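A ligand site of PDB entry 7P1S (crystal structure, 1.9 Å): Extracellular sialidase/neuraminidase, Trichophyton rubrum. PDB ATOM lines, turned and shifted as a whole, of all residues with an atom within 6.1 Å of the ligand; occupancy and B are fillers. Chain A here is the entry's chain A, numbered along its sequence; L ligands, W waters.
OE1 of Gln 128 lies within hydrogen-bond range of O6 of the ligand (2.7 Å).
NH1 of Arg 40 lies within salt-bridge range of O3 of the ligand (3.0 Å).
The side-chain hydroxyl (OH) of Tyr 338 lies close to an oxygen (O5) of the ligand (3.1 Å).
An oxygen (O2) of the ligand is in salt-bridge range of the guanidinium group of Arg 245 (2.9 Å).
NH2 of Arg 302 is in salt-bridge range of O2 of the ligand, 3.0 Å away.
NE1 of Trp 182 is in hydrogen-bond range of O8 of the ligand, 3.2 Å away.
The guanidinium group (NH2) of Arg 59 lies within hydrogen-bond range of an oxygen (O4) of the ligand (2.9 Å).
The side-chain carboxylate of Asp 65 sits close to an oxygen (O4) of the ligand (3.4 Å).
The guanidinium group (NE) of Arg 302 is in hydrogen-bond range of the side-chain sulfur (SG) of Cys 276.
OE1 of Glu 229 is in salt-bridge range of NH1 of Arg 245 (2.8 Å).
The backbone carbonyl oxygen (O) of Arg 40 lies within hydrogen-bond range of the backbone NH (N) of Glu 57, at 2.7 Å.
NH1 of Arg 245 sits at hydrogen-bond distance from OH of Tyr 338 (2.6 Å).
The guanidinium group (NH2) of Arg 302 is in hydrogen-bond range of the backbone carbonyl oxygen (O) of Ala 275 (3.2 Å).
The side-chain carboxylate of Glu 354 lies within hydrogen-bond range of the backbone NH of Tyr 338, at 2.9 Å.
NH1 of Arg 40 is in salt-bridge range of OD1 of Asp 65, at 3.8 Å.
OH of Tyr 338 sits at hydrogen-bond distance from OE2 of Glu 229.
Merely in contact with the ligand: Glu 229 (3.5 Å).
Hydrophobic or aromatic side chains that line the ligand: Trp 182 and Tyr 338.
Nine residues have an atom within 4 Å of the ligand: Arg 40, Arg 59, Asp 65, Gln 128, Trp 182, Glu 229, Arg 245, Arg 302 and Tyr 338.
Water W3 lies within hydrogen-bond range of O4 of the ligand (2.6 Å), OE2 of Glu 57 (2.6 Å) and OD1 of Asn 105 (2.8 Å).
Water W1 bridges an oxygen (O1) of the ligand and the guanidinium group of Arg 151.
Water W4 lies within hydrogen-bond range of the side-chain carboxylate (OE2) of Glu 229 (2.6 Å), an oxygen (O1) of the ligand (2.9 Å) and the side-chain amide nitrogen (ND2) of Asn 105 (2.9 Å).
Water W2 lies within hydrogen-bond range of the side-chain hydroxyl (OG) of Ser 228 (2.6 Å), an oxygen (O7) of the ligand (2.9 Å) and the indole nitrogen (NE1) of Trp 182 (3.1 Å).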
ATOM      1  N   ARG A  40     -18.284 -15.049  19.900  1.00  0.00           N
ATOM      2  CA  ARG A  40     -18.925 -15.911  18.934  1.00  0.00           C
ATOM      3  C   ARG A  40     -17.883 -16.417  17.875  1.00  0.00           C
ATOM      4  O   ARG A  40     -16.720 -16.029  17.876  1.00  0.00           O
ATOM      5  CB  ARG A  40     -20.035 -15.153  18.198  1.00  0.00           C
ATOM      6  CG  ARG A  40     -21.209 -14.690  19.055  1.00  0.00           C
ATOM      7  CD  ARG A  40     -22.464 -14.502  18.196  1.00  0.00           C
ATOM      8  NE  ARG A  40     -22.661 -15.666  17.336  1.00  0.00           N
ATOM      9  CZ  ARG A  40     -23.434 -15.714  16.249  1.00  0.00           C
ATOM     10  NH1 ARG A  40     -24.157 -14.647  15.882  1.00  0.00           N
ATOM     11  NH2 ARG A  40     -23.463 -16.845  15.509  1.00  0.00           N
ATOM     12  N   ILE A  41     -18.339 -17.320  17.031  1.00  0.00           N
ATOM     13  CA  ILE A  41     -17.665 -17.725  15.824  1.00  0.00           C
ATOM     14  C   ILE A  41     -16.323 -18.335  16.144  1.00  0.00           C
ATOM     15  O   ILE A  41     -15.308 -17.738  15.852  1.00  0.00           O
ATOM     16  CB  ILE A  41     -17.483 -16.549  14.847  1.00  0.00           C
ATOM     17  CG1 ILE A  41     -18.672 -15.593  14.887  1.00  0.00           C
ATOM     18  CG2 ILE A  41     -17.269 -17.081  13.430  1.00  0.00           C
ATOM     19  CD1 ILE A  41     -20.010 -16.178  14.492  1.00  0.00           C
ATOM     20  N   GLU A  57     -14.416 -14.562  17.667  1.00  0.00           N
ATOM     21  CA  GLU A  57     -14.696 -13.160  17.518  1.00  0.00           C
ATOM     22  C   GLU A  57     -15.007 -12.638  18.930  1.00  0.00           C
ATOM     23  O   GLU A  57     -15.929 -13.130  19.569  1.00  0.00           O
ATOM     24  CB  GLU A  57     -15.902 -12.927  16.602  1.00  0.00           C
ATOM     25  CG  GLU A  57     -15.573 -12.842  15.106  1.00  0.00           C
ATOM     26  CD  GLU A  57     -16.803 -12.694  14.211  1.00  0.00           C
ATOM     27  OE1 GLU A  57     -17.814 -12.093  14.659  1.00  0.00           O
ATOM     28  OE2 GLU A  57     -16.760 -13.214  13.064  1.00  0.00           O
ATOM     29  N   ARG A  59     -16.684  -9.782  20.394  1.00  0.00           N
ATOM     30  CA  ARG A  59     -17.584  -8.717  20.008  1.00  0.00           C
ATOM     31  C   ARG A  59     -17.690  -7.725  21.170  1.00  0.00           C
ATOM     32  O   ARG A  59     -18.213  -8.073  22.234  1.00  0.00           O
ATOM     33  CB  ARG A  59     -18.929  -9.335  19.651  1.00  0.00           C
ATOM     34  CG  ARG A  59     -18.778 -10.419  18.575  1.00  0.00           C
ATOM     35  CD  ARG A  59     -20.076 -10.799  17.936  1.00  0.00           C
ATOM     36  NE  ARG A  59     -19.812 -11.446  16.646  1.00  0.00           N
ATOM     37  CZ  ARG A  59     -20.752 -11.893  15.830  1.00  0.00           C
ATOM     38  NH1 ARG A  59     -22.045 -11.842  16.168  1.00  0.00           N
ATOM     39  NH2 ARG A  59     -20.387 -12.395  14.670  1.00  0.00           N
ATOM     40  N   ASP A  65     -23.045  -8.924  14.564  1.00  0.00           N
ATOM     41  CA  ASP A  65     -21.999  -9.329  13.605  1.00  0.00           C
ATOM     42  C   ASP A  65     -21.105  -8.195  13.143  1.00  0.00           C
ATOM     43  O   ASP A  65     -20.057  -8.440  12.546  1.00  0.00           O
ATOM     44  CB  ASP A  65     -22.630  -9.920  12.343  1.00  0.00           C
ATOM     45  CG  ASP A  65     -23.667 -10.986  12.639  1.00  0.00           C
ATOM     46  OD1 ASP A  65     -23.690 -11.528  13.764  1.00  0.00           O
ATOM     47  OD2 ASP A  65     -24.446 -11.315  11.740  1.00  0.00           O
ATOM     48  N   ASN A 105     -14.652 -14.169  11.421  1.00  0.00           N
ATOM     49  CA  ASN A 105     -14.688 -15.400  10.635  1.00  0.00           C
ATOM     50  C   ASN A 105     -13.312 -16.099  10.668  1.00  0.00           C
ATOM     51  O   ASN A 105     -12.667 -16.265   9.625  1.00  0.00           O
ATOM     52  CB  ASN A 105     -15.066 -15.132   9.150  1.00  0.00           C
ATOM     53  CG  ASN A 105     -16.550 -14.852   8.950  1.00  0.00           C
ATOM     54  OD1 ASN A 105     -17.046 -13.836   9.383  1.00  0.00           O
ATOM     55  ND2 ASN A 105     -17.236 -15.732   8.236  1.00  0.00           N
ATOM     56  N   GLN A 128     -23.870  -5.839   7.201  1.00  0.00           N
ATOM     57  CA  GLN A 128     -24.455  -6.624   6.140  1.00  0.00           C
ATOM     58  C   GLN A 128     -25.702  -5.969   5.582  1.00  0.00           C
ATOM     59  O   GLN A 128     -25.789  -5.683   4.384  1.00  0.00           O
ATOM     60  CB  GLN A 128     -24.769  -8.026   6.648  1.00  0.00           C
ATOM     61  CG  GLN A 128     -25.341  -8.955   5.593  1.00  0.00           C
ATOM     62  CD  GLN A 128     -25.102 -10.407   5.881  1.00  0.00           C
ATOM     63  OE1 GLN A 128     -25.015 -10.813   7.042  1.00  0.00           O
ATOM     64  NE2 GLN A 128     -24.985 -11.209   4.811  1.00  0.00           N
ATOM     65  N   ARG A 151     -16.676  -6.524   2.116  1.00  0.00           N
ATOM     66  CA  ARG A 151     -16.003  -7.470   3.034  1.00  0.00           C
ATOM     67  C   ARG A 151     -14.652  -7.929   2.474  1.00  0.00           C
ATOM     68  O   ARG A 151     -14.564  -8.457   1.370  1.00  0.00           O
ATOM     69  CB  ARG A 151     -16.899  -8.667   3.321  1.00  0.00           C
ATOM     70  CG  ARG A 151     -18.108  -8.298   4.197  1.00  0.00           C
ATOM     71  CD  ARG A 151     -17.843  -8.597   5.664  1.00  0.00           C
ATOM     72  NE  ARG A 151     -17.903 -10.020   5.962  1.00  0.00           N
ATOM     73  CZ  ARG A 151     -17.645 -10.551   7.170  1.00  0.00           C
ATOM     74  NH1 ARG A 151     -17.302  -9.775   8.186  1.00  0.00           N
ATOM     75  NH2 ARG A 151     -17.729 -11.857   7.363  1.00  0.00           N
ATOM     76  N   TRP A 182     -20.768  -8.436   0.099  1.00  0.00           N
ATOM     77  CA  TRP A 182     -20.666  -9.404   1.224  1.00  0.00           C
ATOM     78  C   TRP A 182     -19.741 -10.593   0.917  1.00  0.00           C
ATOM     79  O   TRP A 182     -19.623 -11.060  -0.223  1.00  0.00           O
ATOM     80  CB  TRP A 182     -22.034  -9.936   1.628  1.00  0.00           C
ATOM     81  CG  TRP A 182     -21.972 -10.721   2.937  1.00  0.00           C
ATOM     82  CD1 TRP A 182     -22.091 -12.069   3.103  1.00  0.00           C
ATOM     83  CD2 TRP A 182     -21.734 -10.175   4.243  1.00  0.00           C
ATOM     84  NE1 TRP A 182     -21.949 -12.390   4.422  1.00  0.00           N
ATOM     85  CE2 TRP A 182     -21.724 -11.246   5.142  1.00  0.00           C
ATOM     86  CE3 TRP A 182     -21.534  -8.875   4.736  1.00  0.00           C
ATOM     87  CZ2 TRP A 182     -21.532 -11.071   6.518  1.00  0.00           C
ATOM     88  CZ3 TRP A 182     -21.315  -8.695   6.101  1.00  0.00           C
ATOM     89  CH2 TRP A 182     -21.327  -9.789   6.974  1.00  0.00           C
ATOM     90  N   ASP A 183     -19.067 -11.065   1.954  1.00  0.00           N
ATOM     91  CA  ASP A 183     -18.171 -12.187   1.818  1.00  0.00           C
ATOM     92  C   ASP A 183     -18.036 -12.814   3.198  1.00  0.00           C
ATOM     93  O   ASP A 183     -18.373 -12.197   4.230  1.00  0.00           O
ATOM     94  CB  ASP A 183     -16.813 -11.732   1.329  1.00  0.00           C
ATOM     95  CG  ASP A 183     -15.932 -12.883   0.926  1.00  0.00           C
ATOM     96  OD1 ASP A 183     -16.481 -13.880   0.388  1.00  0.00           O
ATOM     97  OD2 ASP A 183     -14.708 -12.812   1.130  1.00  0.00           O
ATOM     98  N   ALA A 184     -17.628 -14.081   3.167  1.00  0.00           N
ATOM     99  CA  ALA A 184     -17.297 -14.839   4.362  1.00  0.00           C
ATOM    100  C   ALA A 184     -16.182 -15.808   3.992  1.00  0.00           C
ATOM    101  O   ALA A 184     -16.162 -16.331   2.869  1.00  0.00           O
ATOM    102  CB  ALA A 184     -18.505 -15.605   4.879  1.00  0.00           C
ATOM    103  N   GLN A 203     -17.161 -18.225   0.875  1.00  0.00           N
ATOM    104  CA  GLN A 203     -18.405 -17.962   0.147  1.00  0.00           C
ATOM    105  C   GLN A 203     -18.196 -18.164  -1.375  1.00  0.00           C
ATOM    106  O   GLN A 203     -17.384 -17.459  -1.990  1.00  0.00           O
ATOM    107  CB  GLN A 203     -18.869 -16.538   0.372  1.00  0.00           C
ATOM    108  CG  GLN A 203     -20.038 -16.145  -0.490  1.00  0.00           C
ATOM    109  CD  GLN A 203     -20.743 -14.941   0.042  1.00  0.00           C
ATOM    110  OE1 GLN A 203     -21.026 -14.851   1.247  1.00  0.00           O
ATOM    111  NE2 GLN A 203     -21.041 -13.967  -0.857  1.00  0.00           N
ATOM    112  N   SER A 228     -22.422 -19.377   1.607  1.00  0.00           N
ATOM    113  CA  SER A 228     -21.531 -18.362   2.141  1.00  0.00           C
ATOM    114  C   SER A 228     -20.586 -18.967   3.193  1.00  0.00           C
ATOM    115  O   SER A 228     -19.381 -18.699   3.185  1.00  0.00           O
ATOM    116  CB  SER A 228     -22.336 -17.208   2.720  1.00  0.00           C
ATOM    117  OG  SER A 228     -21.514 -16.150   3.215  1.00  0.00           O
ATOM    118  N   GLU A 229     -21.149 -19.801   4.102  1.00  0.00           N
ATOM    119  CA  GLU A 229     -20.445 -20.470   5.201  1.00  0.00           C
ATOM    120  C   GLU A 229     -20.258 -21.966   4.953  1.00  0.00           C
ATOM    121  O   GLU A 229     -21.173 -22.769   5.147  1.00  0.00           O
ATOM    122  CB  GLU A 229     -21.179 -20.250   6.527  1.00  0.00           C
ATOM    123  CG  GLU A 229     -20.928 -18.868   7.111  1.00  0.00           C
ATOM    124  CD  GLU A 229     -21.638 -18.600   8.437  1.00  0.00           C
ATOM    125  OE1 GLU A 229     -22.405 -19.454   8.885  1.00  0.00           O
ATOM    126  OE2 GLU A 229     -21.410 -17.523   9.019  1.00  0.00           O
ATOM    127  N   ARG A 245     -23.704 -24.275   4.946  1.00  0.00           N
ATOM    128  CA  ARG A 245     -24.872 -23.691   5.576  1.00  0.00           C
ATOM    129  C   ARG A 245     -25.813 -23.302   4.467  1.00  0.00           C
ATOM    130  O   ARG A 245     -25.371 -22.656   3.518  1.00  0.00           O
ATOM    131  CB  ARG A 245     -24.472 -22.429   6.331  1.00  0.00           C
ATOM    132  CG  ARG A 245     -25.616 -21.592   6.854  1.00  0.00           C
ATOM    133  CD  ARG A 245     -25.073 -20.417   7.625  1.00  0.00           C
ATOM    134  NE  ARG A 245     -26.083 -19.443   7.982  1.00  0.00           N
ATOM    135  CZ  ARG A 245     -25.954 -18.558   8.947  1.00  0.00           C
ATOM    136  NH1 ARG A 245     -24.864 -18.520   9.704  1.00  0.00           N
ATOM    137  NH2 ARG A 245     -26.938 -17.709   9.156  1.00  0.00           N
ATOM    138  N   ALA A 275     -30.116 -23.168   9.205  1.00  0.00           N
ATOM    139  CA  ALA A 275     -29.361 -22.058   8.634  1.00  0.00           C
ATOM    140  C   ALA A 275     -28.375 -21.537   9.652  1.00  0.00           C
ATOM    141  O   ALA A 275     -28.516 -20.434  10.181  1.00  0.00           O
ATOM    142  CB  ALA A 275     -30.285 -20.962   8.129  1.00  0.00           C
ATOM    143  N   CYS A 276     -27.389 -22.364   9.939  1.00  0.00           N
ATOM    144  CA  CYS A 276     -26.357 -22.054  10.906  1.00  0.00           C
ATOM    145  C   CYS A 276     -25.083 -22.719  10.452  1.00  0.00           C
ATOM    146  O   CYS A 276     -25.138 -23.689   9.684  1.00  0.00           O
ATOM    147  CB  CYS A 276     -26.752 -22.563  12.287  1.00  0.00           C
ATOM    148  SG  CYS A 276     -25.694 -22.012  13.618  1.00  0.00           S
ATOM    149  N   ARG A 302     -31.126 -23.486  16.861  1.00  0.00           N
ATOM    150  CA  ARG A 302     -29.707 -23.759  17.010  1.00  0.00           C
ATOM    151  C   ARG A 302     -29.346 -24.583  18.255  1.00  0.00           C
ATOM    152  O   ARG A 302     -28.161 -24.881  18.488  1.00  0.00           O
ATOM    153  CB  ARG A 302     -28.958 -22.414  17.025  1.00  0.00           C
ATOM    154  CG  ARG A 302     -29.213 -21.632  15.734  1.00  0.00           C
ATOM    155  CD  ARG A 302     -28.377 -20.380  15.642  1.00  0.00           C
ATOM    156  NE  ARG A 302     -28.393 -19.846  14.280  1.00  0.00           N
ATOM    157  CZ  ARG A 302     -27.615 -18.872  13.818  1.00  0.00           C
ATOM    158  NH1 ARG A 302     -26.711 -18.267  14.580  1.00  0.00           N
ATOM    159  NH2 ARG A 302     -27.738 -18.501  12.561  1.00  0.00           N
ATOM    160  N   TYR A 338     -22.815 -21.995  16.302  1.00  0.00           N
ATOM    161  CA  TYR A 338     -21.605 -22.246  15.509  1.00  0.00           C
ATOM    162  C   TYR A 338     -20.725 -23.215  16.276  1.00  0.00           C
ATOM    163  O   TYR A 338     -20.724 -23.183  17.527  1.00  0.00           O
ATOM    164  CB  TYR A 338     -20.822 -20.959  15.241  1.00  0.00           C
ATOM    165  CG  TYR A 338     -21.349 -20.078  14.133  1.00  0.00           C
ATOM    166  CD1 TYR A 338     -22.720 -19.809  13.996  1.00  0.00           C
ATOM    167  CD2 TYR A 338     -20.476 -19.489  13.215  1.00  0.00           C
ATOM    168  CE1 TYR A 338     -23.201 -18.994  13.002  1.00  0.00           C
ATOM    169  CE2 TYR A 338     -20.969 -18.656  12.200  1.00  0.00           C
ATOM    170  CZ  TYR A 338     -22.329 -18.422  12.109  1.00  0.00           C
ATOM    171  OH  TYR A 338     -22.828 -17.637  11.104  1.00  0.00           O
ATOM    172  N   GLU A 354     -20.761 -22.576  20.595  1.00  0.00           N
ATOM    173  CA  GLU A 354     -21.371 -21.339  21.036  1.00  0.00           C
ATOM    174  C   GLU A 354     -22.489 -21.608  22.018  1.00  0.00           C
ATOM    175  O   GLU A 354     -23.149 -22.639  21.931  1.00  0.00           O
ATOM    176  CB  GLU A 354     -21.969 -20.581  19.828  1.00  0.00           C
ATOM    177  CG  GLU A 354     -20.974 -19.919  18.889  1.00  0.00           C
ATOM    178  CD  GLU A 354     -21.670 -19.011  17.870  1.00  0.00           C
ATOM    179  OE1 GLU A 354     -22.780 -19.345  17.377  1.00  0.00           O
ATOM    180  OE2 GLU A 354     -21.118 -17.949  17.558  1.00  0.00           O
ATOM    181  N   ARG A 368     -23.111 -13.776  24.672  1.00  0.00           N
ATOM    182  CA  ARG A 368     -22.754 -15.050  24.031  1.00  0.00           C
ATOM    183  C   ARG A 368     -21.398 -15.514  24.533  1.00  0.00           C
ATOM    184  O   ARG A 368     -20.466 -14.721  24.627  1.00  0.00           O
ATOM    185  CB  ARG A 368     -22.679 -14.905  22.524  1.00  0.00           C
ATOM    186  CG  ARG A 368     -23.837 -14.140  21.900  1.00  0.00           C
ATOM    187  CD  ARG A 368     -25.171 -14.853  22.184  1.00  0.00           C
ATOM    188  NE  ARG A 368     -26.273 -14.272  21.438  1.00  0.00           N
ATOM    189  CZ  ARG A 368     -26.573 -14.546  20.174  1.00  0.00           C
ATOM    190  NH1 ARG A 368     -25.821 -15.372  19.448  1.00  0.00           N
ATOM    191  NH2 ARG A 368     -27.622 -13.959  19.606  1.00  0.00           N
HETATM  192  C1  LIG L   1     -25.447 -15.689  12.187  1.00  0.00           C
HETATM  193  C2  LIG L   1     -23.276 -14.532  12.152  1.00  0.00           C
HETATM  194  C3  LIG L   1     -22.080 -14.130  11.328  1.00  0.00           C
HETATM  195  C4  LIG L   1     -22.535 -13.545  10.001  1.00  0.00           C
HETATM  196  C5  LIG L   1     -23.388 -14.591   9.278  1.00  0.00           C
HETATM  197  C6  LIG L   1     -24.133 -14.052   8.061  1.00  0.00           C
HETATM  198  C7  LIG L   1     -24.918 -15.129   7.330  1.00  0.00           C
HETATM  199  C8  LIG L   1     -25.600 -14.606   6.066  1.00  0.00           C
HETATM  200  O1  LIG L   1     -21.375 -13.258   9.200  1.00  0.00           O
HETATM  201  O2  LIG L   1     -26.360 -16.134  11.460  1.00  0.00           O
HETATM  202  O3  LIG L   1     -25.440 -15.838  13.407  1.00  0.00           O
HETATM  203  O4  LIG L   1     -21.291 -13.170  11.989  1.00  0.00           O
HETATM  204  O5  LIG L   1     -24.404 -15.164  10.075  1.00  0.00           O
HETATM  205  C9  LIG L   1     -24.323 -15.064  11.523  1.00  0.00           C
HETATM  206  O6  LIG L   1     -25.038 -13.108   8.548  1.00  0.00           O
HETATM  207  O7  LIG L   1     -24.034 -16.183   7.005  1.00  0.00           O
HETATM  208  O8  LIG L   1     -24.673 -13.993   5.153  1.00  0.00           O
HETATM  209  O   HOH W   1     -19.834 -11.035   9.986  1.00  0.00           O
HETATM  210  O   HOH W   2     -21.624 -15.170   5.660  1.00  0.00           O
HETATM  211  O   HOH W   3     -18.800 -13.884  11.543  1.00  0.00           O
HETATM  212  O   HOH W   4     -20.123 -15.509   7.942  1.00  0.00           O
HETATM  213  O   HOH W   5     -27.007 -13.931  10.102  1.00  0.00           O
